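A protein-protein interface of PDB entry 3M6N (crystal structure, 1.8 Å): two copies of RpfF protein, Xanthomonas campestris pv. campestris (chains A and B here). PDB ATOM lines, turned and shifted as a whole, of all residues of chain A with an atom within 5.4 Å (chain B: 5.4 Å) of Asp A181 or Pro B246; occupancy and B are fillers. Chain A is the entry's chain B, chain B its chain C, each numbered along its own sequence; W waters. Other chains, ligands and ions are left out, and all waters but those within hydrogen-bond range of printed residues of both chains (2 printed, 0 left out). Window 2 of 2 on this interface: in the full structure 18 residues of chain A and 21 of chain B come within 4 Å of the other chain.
ND1 of His B247 is in hydrogen-bond range of OD2 of Asp A181 (2.8 Å).
N of Ala B248 sits at hydrogen-bond distance from OD1 of Asp A181, at 2.8 Å.
O of Ser B242 is in hydrogen-bond range of OG1 of Thr B245, at 3.4 Å.
Water W1 bridges O of Leu A179 (2.7 Å) and O of Arg B244 (2.7 Å).
Water W2 lies within hydrogen-bond range of O of His B247 (2.8 Å) and OG1 of Thr A277 (3.0 Å).
Asp A181 touches just these residues of chain B: Thr B245 (3.3 Å), Pro B246 (3.4 Å), His B247 (2.8 Å) and Ala B248 (2.8 Å).
Pro B246 touches one residue of chain A.
Of the printed residues of chain A, Thr B245 touches Val A178 and Asp A181.
Of the printed residues of chain A, Ala B251 touches Phe A183 (3.7 Å) and Thr A277 (3.5 Å).
Printed residues of chain A within 4 Å of Arg B244: Leu A179 (3.8 Å).
Leu B85 touches none of the printed residues of chain A.
Hydrophobic or aromatic side chains of chain A within 4 Å of the printed part of chain B: Phe A183.
Of the 12 printed residues of chain B, 6 touch a printed residue of chain A.
Printed residues of chain B that touch a printed residue of chain A: Arg B244, Thr B245, Pro B246, His B247, Ala B248 and Ala B251.
Hydrophobic or aromatic side chains of chain B that line the printed part of chain A: Pro B246, His B247, Ala B248 and Ala B251.
Among the printed residues, 10 pairs touch across the chains.
Among the printed residues, no Asp or Glu carboxylate lies within 4 Å of a Lys or Arg side-chain nitrogen of the other chain.
No position is printed for both chains.
Of the 10 pairs that touch across the chains among the printed residues, none has its exchanged pair printed and touching as well.
Among the printed residues, pairs that only touch across the chains: Val A178 with Thr B245 (3.3 Å), Leu A179 with Arg B244 (3.8 Å), Asp A181 with Thr B245 (3.3 Å), Asp A181 with Pro B246 (3.4 Å), Phe A183 with Ala B248 (3.7 Å), Phe A183 with Ala B251 (3.7 Å), Thr A277 with His B247 (3.8 Å) and Thr A277 with Ala B251 (3.5 Å).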
ATOM      1  N   GLU A 177     -29.223  -9.125 -28.123  1.00  0.00           N
ATOM      2  CA  GLU A 177     -28.725  -8.237 -27.076  1.00  0.00           C
ATOM      3  C   GLU A 177     -28.879  -8.851 -25.690  1.00  0.00           C
ATOM      4  O   GLU A 177     -28.120  -8.538 -24.773  1.00  0.00           O
ATOM      5  CB  GLU A 177     -29.437  -6.886 -27.130  1.00  0.00           C
ATOM      6  CG  GLU A 177     -30.936  -6.965 -26.894  1.00  0.00           C
ATOM      7  CD  GLU A 177     -31.657  -5.720 -27.364  1.00  0.00           C
ATOM      8  OE1 GLU A 177     -30.980  -4.801 -27.869  1.00  0.00           O
ATOM      9  OE2 GLU A 177     -32.898  -5.662 -27.234  1.00  0.00           O
ATOM     10  N   VAL A 178     -29.867  -9.727 -25.539  1.00  0.00           N
ATOM     11  CA  VAL A 178     -30.095 -10.388 -24.262  1.00  0.00           C
ATOM     12  C   VAL A 178     -28.850 -11.147 -23.822  1.00  0.00           C
ATOM     13  O   VAL A 178     -28.639 -11.377 -22.631  1.00  0.00           O
ATOM     14  CB  VAL A 178     -31.282 -11.361 -24.337  1.00  0.00           C
ATOM     15  CG1 VAL A 178     -32.540 -10.619 -24.756  1.00  0.00           C
ATOM     16  CG2 VAL A 178     -30.977 -12.495 -25.303  1.00  0.00           C
ATOM     17  N   LEU A 179     -28.023 -11.528 -24.792  1.00  0.00           N
ATOM     18  CA  LEU A 179     -26.821 -12.308 -24.516  1.00  0.00           C
ATOM     19  C   LEU A 179     -25.837 -11.586 -23.595  1.00  0.00           C
ATOM     20  O   LEU A 179     -25.158 -12.225 -22.789  1.00  0.00           O
ATOM     21  CB  LEU A 179     -26.133 -12.728 -25.818  1.00  0.00           C
ATOM     22  CG  LEU A 179     -26.911 -13.728 -26.677  1.00  0.00           C
ATOM     23  CD1 LEU A 179     -26.099 -14.143 -27.895  1.00  0.00           C
ATOM     24  CD2 LEU A 179     -27.306 -14.944 -25.854  1.00  0.00           C
ATOM     25  N   PHE A 180     -25.751 -10.264 -23.713  1.00  0.00           N
ATOM     26  CA  PHE A 180     -24.945  -9.496 -22.766  1.00  0.00           C
ATOM     27  C   PHE A 180     -25.798  -8.920 -21.639  1.00  0.00           C
ATOM     28  O   PHE A 180     -25.456  -7.906 -21.031  1.00  0.00           O
ATOM     29  CB  PHE A 180     -24.087  -8.421 -23.453  1.00  0.00           C
ATOM     30  CG  PHE A 180     -24.818  -7.607 -24.484  1.00  0.00           C
ATOM     31  CD1 PHE A 180     -25.550  -6.493 -24.114  1.00  0.00           C
ATOM     32  CD2 PHE A 180     -24.741  -7.938 -25.827  1.00  0.00           C
ATOM     33  CE1 PHE A 180     -26.210  -5.734 -25.064  1.00  0.00           C
ATOM     34  CE2 PHE A 180     -25.399  -7.184 -26.780  1.00  0.00           C
ATOM     35  CZ  PHE A 180     -26.134  -6.081 -26.398  1.00  0.00           C
ATOM     36  N   ASP A 181     -26.915  -9.592 -21.374  1.00  0.00           N
ATOM     37  CA  ASP A 181     -27.769  -9.290 -20.229  1.00  0.00           C
ATOM     38  C   ASP A 181     -28.525  -7.972 -20.369  1.00  0.00           C
ATOM     39  O   ASP A 181     -28.774  -7.281 -19.381  1.00  0.00           O
ATOM     40  CB  ASP A 181     -26.957  -9.305 -18.931  1.00  0.00           C
ATOM     41  CG  ASP A 181     -27.778  -9.749 -17.738  1.00  0.00           C
ATOM     42  OD1 ASP A 181     -28.956 -10.120 -17.933  1.00  0.00           O
ATOM     43  OD2 ASP A 181     -27.249  -9.734 -16.608  1.00  0.00           O
ATOM     44  N   LEU A 182     -28.889  -7.631 -21.600  1.00  0.00           N
ATOM     45  CA  LEU A 182     -29.721  -6.461 -21.852  1.00  0.00           C
ATOM     46  C   LEU A 182     -31.130  -6.899 -22.234  1.00  0.00           C
ATOM     47  O   LEU A 182     -31.330  -7.538 -23.265  1.00  0.00           O
ATOM     48  CB  LEU A 182     -29.122  -5.599 -22.965  1.00  0.00           C
ATOM     49  CG  LEU A 182     -29.929  -4.367 -23.381  1.00  0.00           C
ATOM     50  CD1 LEU A 182     -30.058  -3.388 -22.224  1.00  0.00           C
ATOM     51  CD2 LEU A 182     -29.296  -3.690 -24.588  1.00  0.00           C
ATOM     52  N   PHE A 183     -32.100  -6.562 -21.392  1.00  0.00           N
ATOM     53  CA  PHE A 183     -33.492  -6.907 -21.651  1.00  0.00           C
ATOM     54  C   PHE A 183     -34.028  -6.112 -22.839  1.00  0.00           C
ATOM     55  O   PHE A 183     -33.847  -4.897 -22.906  1.00  0.00           O
ATOM     56  CB  PHE A 183     -34.342  -6.644 -20.406  1.00  0.00           C
ATOM     57  CG  PHE A 183     -35.788  -7.017 -20.567  1.00  0.00           C
ATOM     58  CD1 PHE A 183     -36.187  -8.340 -20.497  1.00  0.00           C
ATOM     59  CD2 PHE A 183     -36.749  -6.044 -20.781  1.00  0.00           C
ATOM     60  CE1 PHE A 183     -37.516  -8.685 -20.642  1.00  0.00           C
ATOM     61  CE2 PHE A 183     -38.080  -6.384 -20.929  1.00  0.00           C
ATOM     62  CZ  PHE A 183     -38.463  -7.707 -20.859  1.00  0.00           C
ATOM     63  N   THR A 277     -32.922  -2.253 -15.368  1.00  0.00           N
ATOM     64  CA  THR A 277     -32.060  -3.377 -15.708  1.00  0.00           C
ATOM     65  C   THR A 277     -30.832  -2.900 -16.475  1.00  0.00           C
ATOM     66  O   THR A 277     -29.712  -3.340 -16.212  1.00  0.00           O
ATOM     67  CB  THR A 277     -32.810  -4.427 -16.545  1.00  0.00           C
ATOM     68  OG1 THR A 277     -33.828  -5.039 -15.743  1.00  0.00           O
ATOM     69  CG2 THR A 277     -31.853  -5.500 -17.042  1.00  0.00           C
ATOM     70  N   LEU A 281     -26.011  -2.980 -15.916  1.00  0.00           N
ATOM     71  CA  LEU A 281     -25.072  -3.682 -16.787  1.00  0.00           C
ATOM     72  C   LEU A 281     -23.642  -3.589 -16.262  1.00  0.00           C
ATOM     73  O   LEU A 281     -23.170  -2.510 -15.901  1.00  0.00           O
ATOM     74  CB  LEU A 281     -25.151  -3.139 -18.216  1.00  0.00           C
ATOM     75  CG  LEU A 281     -26.348  -3.605 -19.048  1.00  0.00           C
ATOM     76  CD1 LEU A 281     -26.476  -2.785 -20.323  1.00  0.00           C
ATOM     77  CD2 LEU A 281     -26.234  -5.089 -19.369  1.00  0.00           C
ATOM     78  N   SER A 285     -20.394  -6.678 -19.952  1.00  0.00           N
ATOM     79  CA  SER A 285     -21.466  -6.389 -20.898  1.00  0.00           C
ATOM     80  C   SER A 285     -21.205  -5.091 -21.655  1.00  0.00           C
ATOM     81  O   SER A 285     -21.311  -5.045 -22.880  1.00  0.00           O
ATOM     82  CB  SER A 285     -22.816  -6.315 -20.178  1.00  0.00           C
ATOM     83  OG  SER A 285     -23.177  -7.576 -19.643  1.00  0.00           O
ATOM     84  N   LEU B  85     -29.829 -12.921  -7.235  1.00  0.00           N
ATOM     85  CA  LEU B  85     -30.462 -12.609  -8.509  1.00  0.00           C
ATOM     86  C   LEU B  85     -30.621 -13.844  -9.392  1.00  0.00           C
ATOM     87  O   LEU B  85     -29.643 -14.513  -9.726  1.00  0.00           O
ATOM     88  CB  LEU B  85     -29.660 -11.536  -9.253  1.00  0.00           C
ATOM     89  CG  LEU B  85     -30.269 -11.010 -10.556  1.00  0.00           C
ATOM     90  CD1 LEU B  85     -31.627 -10.380 -10.292  1.00  0.00           C
ATOM     91  CD2 LEU B  85     -29.333 -10.016 -11.228  1.00  0.00           C
ATOM     92  N   ALA B  86     -31.863 -14.140  -9.759  1.00  0.00           N
ATOM     93  CA  ALA B  86     -32.158 -15.216 -10.702  1.00  0.00           C
ATOM     94  C   ALA B  86     -31.645 -16.579 -10.243  1.00  0.00           C
ATOM     95  O   ALA B  86     -30.847 -17.208 -10.934  1.00  0.00           O
ATOM     96  CB  ALA B  86     -31.601 -14.876 -12.076  1.00  0.00           C
ATOM     97  N   SER B 242     -28.995 -19.856 -18.822  1.00  0.00           N
ATOM     98  CA  SER B 242     -29.755 -18.866 -18.068  1.00  0.00           C
ATOM     99  C   SER B 242     -28.873 -18.009 -17.164  1.00  0.00           C
ATOM    100  O   SER B 242     -29.045 -16.792 -17.094  1.00  0.00           O
ATOM    101  CB  SER B 242     -30.851 -19.550 -17.244  1.00  0.00           C
ATOM    102  OG  SER B 242     -30.304 -20.522 -16.371  1.00  0.00           O
ATOM    103  N   LYS B 243     -27.933 -18.646 -16.473  1.00  0.00           N
ATOM    104  CA  LYS B 243     -27.062 -17.937 -15.539  1.00  0.00           C
ATOM    105  C   LYS B 243     -26.252 -16.838 -16.222  1.00  0.00           C
ATOM    106  O   LYS B 243     -25.702 -15.958 -15.560  1.00  0.00           O
ATOM    107  CB  LYS B 243     -26.129 -18.912 -14.813  1.00  0.00           C
ATOM    108  CG  LYS B 243     -26.834 -19.810 -13.808  1.00  0.00           C
ATOM    109  CD  LYS B 243     -25.844 -20.684 -13.052  1.00  0.00           C
ATOM    110  CE  LYS B 243     -24.946 -19.853 -12.149  1.00  0.00           C
ATOM    111  NZ  LYS B 243     -25.717 -19.168 -11.074  1.00  0.00           N
ATOM    112  N   ARG B 244     -26.181 -16.894 -17.547  1.00  0.00           N
ATOM    113  CA  ARG B 244     -25.432 -15.903 -18.312  1.00  0.00           C
ATOM    114  C   ARG B 244     -26.280 -14.674 -18.629  1.00  0.00           C
ATOM    115  O   ARG B 244     -25.876 -13.817 -19.415  1.00  0.00           O
ATOM    116  CB  ARG B 244     -24.889 -16.521 -19.603  1.00  0.00           C
ATOM    117  CG  ARG B 244     -25.952 -17.160 -20.482  1.00  0.00           C
ATOM    118  CD  ARG B 244     -25.338 -17.852 -21.692  1.00  0.00           C
ATOM    119  NE  ARG B 244     -24.566 -19.037 -21.323  1.00  0.00           N
ATOM    120  CZ  ARG B 244     -23.240 -19.070 -21.241  1.00  0.00           C
ATOM    121  NH1 ARG B 244     -22.529 -17.983 -21.506  1.00  0.00           N
ATOM    122  NH2 ARG B 244     -22.623 -20.193 -20.896  1.00  0.00           N
ATOM    123  N   THR B 245     -27.454 -14.591 -18.010  1.00  0.00           N
ATOM    124  CA  THR B 245     -28.350 -13.460 -18.229  1.00  0.00           C
ATOM    125  C   THR B 245     -29.333 -13.300 -17.072  1.00  0.00           C
ATOM    126  O   THR B 245     -30.547 -13.338 -17.271  1.00  0.00           O
ATOM    127  CB  THR B 245     -29.132 -13.615 -19.544  1.00  0.00           C
ATOM    128  OG1 THR B 245     -30.152 -14.610 -19.384  1.00  0.00           O
ATOM    129  CG2 THR B 245     -28.197 -14.027 -20.669  1.00  0.00           C
ATOM    130  N   PRO B 246     -28.803 -13.111 -15.853  1.00  0.00           N
ATOM    131  CA  PRO B 246     -29.599 -13.014 -14.630  1.00  0.00           C
ATOM    132  C   PRO B 246     -30.503 -11.784 -14.593  1.00  0.00           C
ATOM    133  O   PRO B 246     -31.667 -11.887 -14.210  1.00  0.00           O
ATOM    134  CB  PRO B 246     -28.539 -12.924 -13.528  1.00  0.00           C
ATOM    135  CG  PRO B 246     -27.327 -12.392 -14.209  1.00  0.00           C
ATOM    136  CD  PRO B 246     -27.361 -12.976 -15.586  1.00  0.00           C
ATOM    137  N   HIS B 247     -29.970 -10.629 -14.979  1.00  0.00           N
ATOM    138  CA  HIS B 247     -30.749  -9.396 -14.950  1.00  0.00           C
ATOM    139  C   HIS B 247     -31.895  -9.430 -15.958  1.00  0.00           C
ATOM    140  O   HIS B 247     -33.001  -8.975 -15.667  1.00  0.00           O
ATOM    141  CB  HIS B 247     -29.857  -8.179 -15.196  1.00  0.00           C
ATOM    142  CG  HIS B 247     -28.855  -7.935 -14.112  1.00  0.00           C
ATOM    143  ND1 HIS B 247     -27.499  -8.092 -14.301  1.00  0.00           N
ATOM    144  CD2 HIS B 247     -29.012  -7.551 -12.822  1.00  0.00           C
ATOM    145  CE1 HIS B 247     -26.864  -7.810 -13.178  1.00  0.00           C
ATOM    146  NE2 HIS B 247     -27.758  -7.479 -12.265  1.00  0.00           N
ATOM    147  N   ALA B 248     -31.623  -9.969 -17.142  1.00  0.00           N
ATOM    148  CA  ALA B 248     -32.642 -10.089 -18.177  1.00  0.00           C
ATOM    149  C   ALA B 248     -33.762 -11.017 -17.722  1.00  0.00           C
ATOM    150  O   ALA B 248     -34.937 -10.774 -17.999  1.00  0.00           O
ATOM    151  CB  ALA B 248     -32.027 -10.589 -19.475  1.00  0.00           C
ATOM    152  N   TRP B 249     -33.393 -12.083 -17.018  1.00  0.00           N
ATOM    153  CA  TRP B 249     -34.380 -13.012 -16.485  1.00  0.00           C
ATOM    154  C   TRP B 249     -35.276 -12.324 -15.462  1.00  0.00           C
ATOM    155  O   TRP B 249     -36.500 -12.434 -15.522  1.00  0.00           O
ATOM    156  CB  TRP B 249     -33.700 -14.223 -15.846  1.00  0.00           C
ATOM    157  CG  TRP B 249     -34.642 -15.050 -15.029  1.00  0.00           C
ATOM    158  CD1 TRP B 249     -34.864 -14.955 -13.686  1.00  0.00           C
ATOM    159  CD2 TRP B 249     -35.505 -16.088 -15.506  1.00  0.00           C
ATOM    160  NE1 TRP B 249     -35.805 -15.875 -13.295  1.00  0.00           N
ATOM    161  CE2 TRP B 249     -36.215 -16.583 -14.394  1.00  0.00           C
ATOM    162  CE3 TRP B 249     -35.743 -16.651 -16.763  1.00  0.00           C
ATOM    163  CZ2 TRP B 249     -37.146 -17.614 -14.503  1.00  0.00           C
ATOM    164  CZ3 TRP B 249     -36.669 -17.673 -16.869  1.00  0.00           C
ATOM    165  CH2 TRP B 249     -37.358 -18.144 -15.745  1.00  0.00           C
ATOM    166  N   ALA B 250     -34.656 -11.617 -14.522  1.00  0.00           N
ATOM    167  CA  ALA B 250     -35.400 -10.904 -13.491  1.00  0.00           C
ATOM    168  C   ALA B 250     -36.382  -9.924 -14.120  1.00  0.00           C
ATOM    169  O   ALA B 250     -37.536  -9.834 -13.705  1.00  0.00           O
ATOM    170  CB  ALA B 250     -34.447 -10.179 -12.556  1.00  0.00           C
ATOM    171  N   ALA B 251     -35.914  -9.192 -15.126  1.00  0.00           N
ATOM    172  CA  ALA B 251     -36.759  -8.241 -15.836  1.00  0.00           C
ATOM    173  C   ALA B 251     -37.958  -8.945 -16.467  1.00  0.00           C
ATOM    174  O   ALA B 251     -39.095  -8.485 -16.344  1.00  0.00           O
ATOM    175  CB  ALA B 251     -35.955  -7.506 -16.894  1.00  0.00           C
HETATM  176  O   HOH W   1     -24.194 -11.826 -20.259  1.00  0.00           O
HETATM  177  O   HOH W   2     -32.960  -7.069 -13.677  1.00  0.00           O
